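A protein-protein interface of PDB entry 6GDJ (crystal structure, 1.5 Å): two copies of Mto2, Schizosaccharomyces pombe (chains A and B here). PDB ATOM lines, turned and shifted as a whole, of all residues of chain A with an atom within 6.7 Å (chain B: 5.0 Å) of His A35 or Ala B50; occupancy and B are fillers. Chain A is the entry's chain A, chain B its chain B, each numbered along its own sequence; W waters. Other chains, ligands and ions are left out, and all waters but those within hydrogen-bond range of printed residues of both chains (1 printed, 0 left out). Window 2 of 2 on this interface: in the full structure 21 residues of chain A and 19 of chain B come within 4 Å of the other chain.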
ATOM      1  N   GLU A  30     -19.000   1.697  -1.324  1.00  0.00           N
ATOM      2  CA  GLU A  30     -20.116   0.745  -1.449  1.00  0.00           C
ATOM      3  C   GLU A  30     -19.681  -0.678  -1.810  1.00  0.00           C
ATOM      4  O   GLU A  30     -20.185  -1.674  -1.298  1.00  0.00           O
ATOM      5  CB  GLU A  30     -21.073   1.243  -2.530  1.00  0.00           C
ATOM      6  CG  GLU A  30     -21.784   2.549  -2.189  1.00  0.00           C
ATOM      7  CD  GLU A  30     -23.212   2.404  -1.754  1.00  0.00           C
ATOM      8  OE1 GLU A  30     -23.633   1.250  -1.497  1.00  0.00           O
ATOM      9  OE2 GLU A  30     -23.814   3.506  -1.532  1.00  0.00           O
ATOM     10  N   GLN A  31     -18.711  -0.751  -2.697  1.00  0.00           N
ATOM     11  CA  GLN A  31     -18.230  -2.063  -3.125  1.00  0.00           C
ATOM     12  C   GLN A  31     -17.522  -2.782  -1.942  1.00  0.00           C
ATOM     13  O   GLN A  31     -17.737  -3.960  -1.726  1.00  0.00           O
ATOM     14  CB  GLN A  31     -17.317  -1.928  -4.338  1.00  0.00           C
ATOM     15  CG  GLN A  31     -18.005  -1.413  -5.565  1.00  0.00           C
ATOM     16  CD  GLN A  31     -18.768  -2.441  -6.265  1.00  0.00           C
ATOM     17  OE1 GLN A  31     -18.950  -3.545  -5.736  1.00  0.00           O
ATOM     18  NE2 GLN A  31     -19.212  -2.123  -7.504  1.00  0.00           N
ATOM     19  N   ALA A  32     -16.730  -2.002  -1.188  1.00  0.00           N
ATOM     20  CA  ALA A  32     -16.043  -2.608  -0.018  1.00  0.00           C
ATOM     21  C   ALA A  32     -17.034  -3.115   1.042  1.00  0.00           C
ATOM     22  O   ALA A  32     -16.908  -4.198   1.547  1.00  0.00           O
ATOM     23  CB  ALA A  32     -15.070  -1.654   0.596  1.00  0.00           C
ATOM     24  N   VAL A  33     -18.035  -2.298   1.303  1.00  0.00           N
ATOM     25  CA  VAL A  33     -19.072  -2.677   2.252  1.00  0.00           C
ATOM     26  C   VAL A  33     -19.787  -3.924   1.776  1.00  0.00           C
ATOM     27  O   VAL A  33     -20.041  -4.836   2.527  1.00  0.00           O
ATOM     28  CB  VAL A  33     -20.038  -1.530   2.518  1.00  0.00           C
ATOM     29  CG1 VAL A  33     -21.286  -2.017   3.300  1.00  0.00           C
ATOM     30  CG2 VAL A  33     -19.366  -0.462   3.316  1.00  0.00           C
ATOM     31  N   ASN A  34     -20.082  -3.947   0.482  1.00  0.00           N
ATOM     32  CA  ASN A  34     -20.695  -5.083  -0.086  1.00  0.00           C
ATOM     33  C   ASN A  34     -19.894  -6.400   0.011  1.00  0.00           C
ATOM     34  O   ASN A  34     -20.410  -7.465   0.339  1.00  0.00           O
ATOM     35  CB  ASN A  34     -21.096  -4.745  -1.490  1.00  0.00           C
ATOM     36  CG  ASN A  34     -22.015  -5.706  -1.998  1.00  0.00           C
ATOM     37  OD1 ASN A  34     -23.225  -5.769  -1.566  1.00  0.00           O
ATOM     38  ND2 ASN A  34     -21.455  -6.586  -2.794  1.00  0.00           N
ATOM     39  N   HIS A  35     -18.567  -6.320  -0.229  1.00  0.00           N
ATOM     40  CA  HIS A  35     -17.739  -7.476  -0.018  1.00  0.00           C
ATOM     41  C   HIS A  35     -17.665  -7.873   1.460  1.00  0.00           C
ATOM     42  O   HIS A  35     -17.616  -9.059   1.768  1.00  0.00           O
ATOM     43  CB  HIS A  35     -16.329  -7.259  -0.601  1.00  0.00           C
ATOM     44  CG  HIS A  35     -16.319  -7.089  -2.074  1.00  0.00           C
ATOM     45  ND1 HIS A  35     -17.009  -7.942  -2.911  1.00  0.00           N
ATOM     46  CD2 HIS A  35     -15.782  -6.125  -2.856  1.00  0.00           C
ATOM     47  CE1 HIS A  35     -16.830  -7.550  -4.164  1.00  0.00           C
ATOM     48  NE2 HIS A  35     -16.088  -6.447  -4.162  1.00  0.00           N
ATOM     49  N   ALA A  36     -17.704  -6.888   2.371  1.00  0.00           N
ATOM     50  CA  ALA A  36     -17.752  -7.215   3.783  1.00  0.00           C
ATOM     51  C   ALA A  36     -18.995  -7.972   4.147  1.00  0.00           C
ATOM     52  O   ALA A  36     -18.955  -8.930   4.925  1.00  0.00           O
ATOM     53  CB  ALA A  36     -17.589  -5.958   4.626  1.00  0.00           C
ATOM     54  N   ILE A  37     -20.108  -7.563   3.593  1.00  0.00           N
ATOM     55  CA  ILE A  37     -21.366  -8.312   3.828  1.00  0.00           C
ATOM     56  C   ILE A  37     -21.217  -9.776   3.356  1.00  0.00           C
ATOM     57  O   ILE A  37     -21.607 -10.706   4.044  1.00  0.00           O
ATOM     58  CB  ILE A  37     -22.580  -7.642   3.156  1.00  0.00           C
ATOM     59  CG1 ILE A  37     -22.810  -6.260   3.770  1.00  0.00           C
ATOM     60  CG2 ILE A  37     -23.801  -8.527   3.218  1.00  0.00           C
ATOM     61  CD1 ILE A  37     -23.754  -5.371   2.987  1.00  0.00           C
ATOM     62  N   THR A  38     -20.632  -9.957   2.152  1.00  0.00           N
ATOM     63  CA  THR A  38     -20.386 -11.305   1.659  1.00  0.00           C
ATOM     64  C   THR A  38     -19.573 -12.104   2.647  1.00  0.00           C
ATOM     65  O   THR A  38     -19.874 -13.245   2.915  1.00  0.00           O
ATOM     66  CB  THR A  38     -19.749 -11.285   0.286  1.00  0.00           C
ATOM     67  OG1 THR A  38     -20.552 -10.538  -0.590  1.00  0.00           O
ATOM     68  CG2 THR A  38     -19.491 -12.676  -0.242  1.00  0.00           C
ATOM     69  N   LEU A  39     -18.493 -11.483   3.184  1.00  0.00           N
ATOM     70  CA  LEU A  39     -17.656 -12.203   4.140  1.00  0.00           C
ATOM     71  C   LEU A  39     -18.391 -12.522   5.462  1.00  0.00           C
ATOM     72  O   LEU A  39     -18.220 -13.579   6.006  1.00  0.00           O
ATOM     73  CB  LEU A  39     -16.404 -11.357   4.460  1.00  0.00           C
ATOM     74  CG  LEU A  39     -15.409 -11.215   3.309  1.00  0.00           C
ATOM     75  CD1 LEU A  39     -14.420 -10.136   3.507  1.00  0.00           C
ATOM     76  CD2 LEU A  39     -14.746 -12.541   3.075  1.00  0.00           C
ATOM     77  N   VAL A  40     -19.235 -11.618   5.968  1.00  0.00           N
ATOM     78  CA  VAL A  40     -20.034 -11.943   7.169  1.00  0.00           C
ATOM     79  C   VAL A  40     -20.901 -13.155   6.895  1.00  0.00           C
ATOM     80  O   VAL A  40     -21.053 -13.997   7.732  1.00  0.00           O
ATOM     81  CB  VAL A  40     -20.913 -10.750   7.533  1.00  0.00           C
ATOM     82  CG1 VAL A  40     -21.968 -11.136   8.554  1.00  0.00           C
ATOM     83  CG2 VAL A  40     -20.102  -9.582   8.030  1.00  0.00           C
ATOM     84  N   THR A  42     -20.517 -15.586   4.536  1.00  0.00           N
ATOM     85  CA  THR A  42     -19.860 -16.778   4.010  1.00  0.00           C
ATOM     86  C   THR A  42     -18.672 -17.284   4.815  1.00  0.00           C
ATOM     87  O   THR A  42     -18.380 -18.466   4.781  1.00  0.00           O
ATOM     88  CB  THR A  42     -19.361 -16.569   2.567  1.00  0.00           C
ATOM     89  OG1 THR A  42     -18.382 -15.540   2.560  1.00  0.00           O
ATOM     90  CG2 THR A  42     -20.475 -16.184   1.602  1.00  0.00           C
ATOM     91  N   VAL A  48     -13.375 -10.416  10.277  1.00  0.00           N
ATOM     92  CA  VAL A  48     -14.435  -9.816   9.411  1.00  0.00           C
ATOM     93  C   VAL A  48     -15.265  -8.804  10.271  1.00  0.00           C
ATOM     94  O   VAL A  48     -15.650  -7.725   9.811  1.00  0.00           O
ATOM     95  CB  VAL A  48     -15.319 -10.945   8.833  1.00  0.00           C
ATOM     96  CG1 VAL A  48     -16.542 -10.362   8.158  1.00  0.00           C
ATOM     97  CG2 VAL A  48     -14.499 -11.832   7.885  1.00  0.00           C
ATOM     98  N   LEU A  51     -13.290  -5.705  10.360  1.00  0.00           N
ATOM     99  CA  LEU A  51     -13.365  -5.056   9.080  1.00  0.00           C
ATOM    100  C   LEU A  51     -14.635  -4.212   9.010  1.00  0.00           C
ATOM    101  O   LEU A  51     -14.607  -3.068   8.571  1.00  0.00           O
ATOM    102  CB  LEU A  51     -13.352  -6.075   7.968  1.00  0.00           C
ATOM    103  CG  LEU A  51     -13.691  -5.567   6.569  1.00  0.00           C
ATOM    104  CD1 LEU A  51     -12.601  -4.642   6.086  1.00  0.00           C
ATOM    105  CD2 LEU A  51     -13.906  -6.706   5.629  1.00  0.00           C
ATOM    106  N   LEU A  55     -15.033  -0.177   8.418  1.00  0.00           N
ATOM    107  CA  LEU A  55     -15.755   0.467   7.374  1.00  0.00           C
ATOM    108  C   LEU A  55     -16.831   1.358   7.867  1.00  0.00           C
ATOM    109  O   LEU A  55     -17.038   2.431   7.310  1.00  0.00           O
ATOM    110  CB  LEU A  55     -16.264  -0.607   6.422  1.00  0.00           C
ATOM    111  CG  LEU A  55     -15.232  -1.366   5.594  1.00  0.00           C
ATOM    112  CD1 LEU A  55     -15.813  -2.556   4.803  1.00  0.00           C
ATOM    113  CD2 LEU A  55     -14.458  -0.403   4.699  1.00  0.00           C
ATOM    114  N   SER B  46     -11.519 -15.243  -3.696  1.00  0.00           N
ATOM    115  CA  SER B  46     -11.850 -14.244  -4.680  1.00  0.00           C
ATOM    116  C   SER B  46     -12.585 -13.073  -4.019  1.00  0.00           C
ATOM    117  O   SER B  46     -12.437 -11.960  -4.488  1.00  0.00           O
ATOM    118  CB  SER B  46     -12.746 -14.813  -5.796  1.00  0.00           C
ATOM    119  OG  SER B  46     -13.788 -15.511  -5.177  1.00  0.00           O
ATOM    120  N   VAL B  47     -13.318 -13.340  -2.927  1.00  0.00           N
ATOM    121  CA  VAL B  47     -14.038 -12.231  -2.236  1.00  0.00           C
ATOM    122  C   VAL B  47     -13.040 -11.335  -1.507  1.00  0.00           C
ATOM    123  O   VAL B  47     -13.148 -10.103  -1.584  1.00  0.00           O
ATOM    124  CB  VAL B  47     -15.173 -12.714  -1.317  1.00  0.00           C
ATOM    125  CG1 VAL B  47     -15.835 -11.565  -0.573  1.00  0.00           C
ATOM    126  CG2 VAL B  47     -16.196 -13.506  -2.134  1.00  0.00           C
ATOM    127  N   VAL B  48     -12.050 -11.957  -0.844  1.00  0.00           N
ATOM    128  CA  VAL B  48     -11.000 -11.142  -0.212  1.00  0.00           C
ATOM    129  C   VAL B  48     -10.225 -10.367  -1.273  1.00  0.00           C
ATOM    130  O   VAL B  48      -9.920  -9.214  -1.088  1.00  0.00           O
ATOM    131  CB  VAL B  48     -10.138 -12.031   0.643  1.00  0.00           C
ATOM    132  CG1 VAL B  48      -8.917 -11.272   1.187  1.00  0.00           C
ATOM    133  CG2 VAL B  48     -10.921 -12.593   1.838  1.00  0.00           C
ATOM    134  N   ASP B  49      -9.935 -10.981  -2.407  1.00  0.00           N
ATOM    135  CA  ASP B  49      -9.253 -10.232  -3.455  1.00  0.00           C
ATOM    136  C   ASP B  49     -10.054  -9.030  -3.935  1.00  0.00           C
ATOM    137  O   ASP B  49      -9.517  -7.967  -4.128  1.00  0.00           O
ATOM    138  CB  ASP B  49      -8.908 -11.102  -4.650  1.00  0.00           C
ATOM    139  CG  ASP B  49      -7.774 -12.093  -4.386  1.00  0.00           C
ATOM    140  OD1 ASP B  49      -6.985 -11.886  -3.466  1.00  0.00           O
ATOM    141  OD2 ASP B  49      -7.656 -13.084  -5.149  1.00  0.00           O
ATOM    142  N   ALA B  50     -11.374  -9.231  -4.059  1.00  0.00           N
ATOM    143  CA  ALA B  50     -12.228  -8.168  -4.516  1.00  0.00           C
ATOM    144  C   ALA B  50     -12.255  -7.056  -3.466  1.00  0.00           C
ATOM    145  O   ALA B  50     -12.313  -5.907  -3.784  1.00  0.00           O
ATOM    146  CB  ALA B  50     -13.614  -8.695  -4.783  1.00  0.00           C
ATOM    147  N   LEU B  51     -12.330  -7.445  -2.214  1.00  0.00           N
ATOM    148  CA  LEU B  51     -12.224  -6.451  -1.151  1.00  0.00           C
ATOM    149  C   LEU B  51     -10.970  -5.603  -1.265  1.00  0.00           C
ATOM    150  O   LEU B  51     -11.021  -4.392  -1.178  1.00  0.00           O
ATOM    151  CB  LEU B  51     -12.283  -7.088   0.196  1.00  0.00           C
ATOM    152  CG  LEU B  51     -12.001  -6.206   1.413  1.00  0.00           C
ATOM    153  CD1 LEU B  51     -13.155  -5.215   1.641  1.00  0.00           C
ATOM    154  CD2 LEU B  51     -11.716  -7.087   2.639  1.00  0.00           C
ATOM    155  N   CYS B  52      -9.840  -6.267  -1.443  1.00  0.00           N
ATOM    156  CA  CYS B  52      -8.586  -5.553  -1.641  1.00  0.00           C
ATOM    157  C   CYS B  52      -8.609  -4.573  -2.818  1.00  0.00           C
ATOM    158  O   CYS B  52      -8.132  -3.474  -2.740  1.00  0.00           O
ATOM    159  CB  CYS B  52      -7.397  -6.504  -1.752  1.00  0.00           C
ATOM    160  SG  CYS B  52      -7.019  -7.479  -0.300  1.00  0.00           S
ATOM    161  N   ARG B  53      -9.176  -5.017  -3.934  1.00  0.00           N
ATOM    162  CA  ARG B  53      -9.329  -4.158  -5.084  1.00  0.00           C
ATOM    163  C   ARG B  53     -10.179  -2.966  -4.764  1.00  0.00           C
ATOM    164  O   ARG B  53      -9.877  -1.854  -5.169  1.00  0.00           O
ATOM    165  CB  ARG B  53      -9.899  -4.895  -6.302  1.00  0.00           C
ATOM    166  CG  ARG B  53      -9.018  -5.969  -6.900  1.00  0.00           C
ATOM    167  CD  ARG B  53      -9.503  -6.389  -8.305  1.00  0.00           C
ATOM    168  NE  ARG B  53      -8.883  -7.666  -8.594  1.00  0.00           N
ATOM    169  CZ  ARG B  53      -9.391  -8.849  -8.261  1.00  0.00           C
ATOM    170  NH1 ARG B  53     -10.635  -8.934  -7.771  1.00  0.00           N
ATOM    171  NH2 ARG B  53      -8.686  -9.964  -8.511  1.00  0.00           N
ATOM    172  N   SER B  54     -11.271  -3.185  -4.000  1.00  0.00           N
ATOM    173  CA  SER B  54     -12.149  -2.079  -3.618  1.00  0.00           C
ATOM    174  C   SER B  54     -11.456  -1.056  -2.716  1.00  0.00           C
ATOM    175  O   SER B  54     -11.604   0.154  -2.851  1.00  0.00           O
ATOM    176  CB  SER B  54     -13.425  -2.569  -2.876  1.00  0.00           C
ATOM    177  OG  SER B  54     -14.177  -3.338  -3.858  1.00  0.00           O
HETATM  178  O   HOH W   1     -14.190  -5.304  -6.164  1.00  0.00           O
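O of Asn A34 sits at hydrogen-bond distance from OG1 of Thr A38 (3.2 Å). The side-chain hydroxyl (OG) of Ser B54 is in hydrogen-bond range of the backbone carbonyl oxygen (O) of Ala B50, at 3.2 Å. O of Thr A38 lies within hydrogen-bond range of OG1 of Thr A42.
Ser B54 touches Gln A31 (OG to CB, 3.5 Å). O of Ala A32 touches CD1 of Leu B51, at 3.9 Å. Ser B54 touches Ala A32 (CB to N, 3.8 Å). Val B47 touches His A35 (CG1 to O, 3.9 Å). His A35 touches Ala B50 (NE2 to CB, 3.4 Å). Leu B51 touches His A35. CD2 of His A35 touches OG of Ser B54, at 3.4 Å. Val B47 touches Thr A38 (CG1 to CG2, 3.8 Å). Leu A39 touches Val B47. Leu B51 touches Leu A51.
Of chain B, only Val B47, Ala B50, Leu B51 and Ser B54 come within 4 Å of His A35. Of the printed residues of chain A, Ala B50 touches His A35. Printed residues of chain A within 4 Å of Ser B54: Gln A31, Ala A32 and His A35. Printed residues of chain A within 4 Å of Val B47: His A35 (3.9 Å), Thr A38 (3.8 Å) and Leu A39 (3.9 Å). Printed residues of chain B within 4 Å of Leu A51: Leu B51. Of the printed residues of chain B, Gln A31 touches Ser B54. Printed residues of chain B within 4 Å of Ala A32: Leu B51 (3.9 Å) and Ser B54 (3.8 Å). The nearest printed residue of chain B that does not touch His A35 is Cys B52 (6.1 Å). The nearest residue of chain A that does not touch Ala B50 is Gln A31 (6.1 Å). The nearest printed residue of chain B that does not touch Ala A32 is Ala B50 (6.2 Å).
Of the 9 printed residues of chain B, 4 touch a printed residue of chain A. Hydrophobic or aromatic side chains of chain B within 4 Å of the printed part of chain A: Val B47, Ala B50 and Leu B51. Among the printed residues, 10 pairs touch across the chains.
Leu B51 touches its own counterpart, Leu A51. Positions printed for both chains: 48 and 51. Of the 10 pairs that touch across the chains among the printed residues, 1 has its exchanged pair printed and touching as well.
Water W1 lies within hydrogen-bond range of NE2 of His A35, OG of Ser B54 and O of Ala B50.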
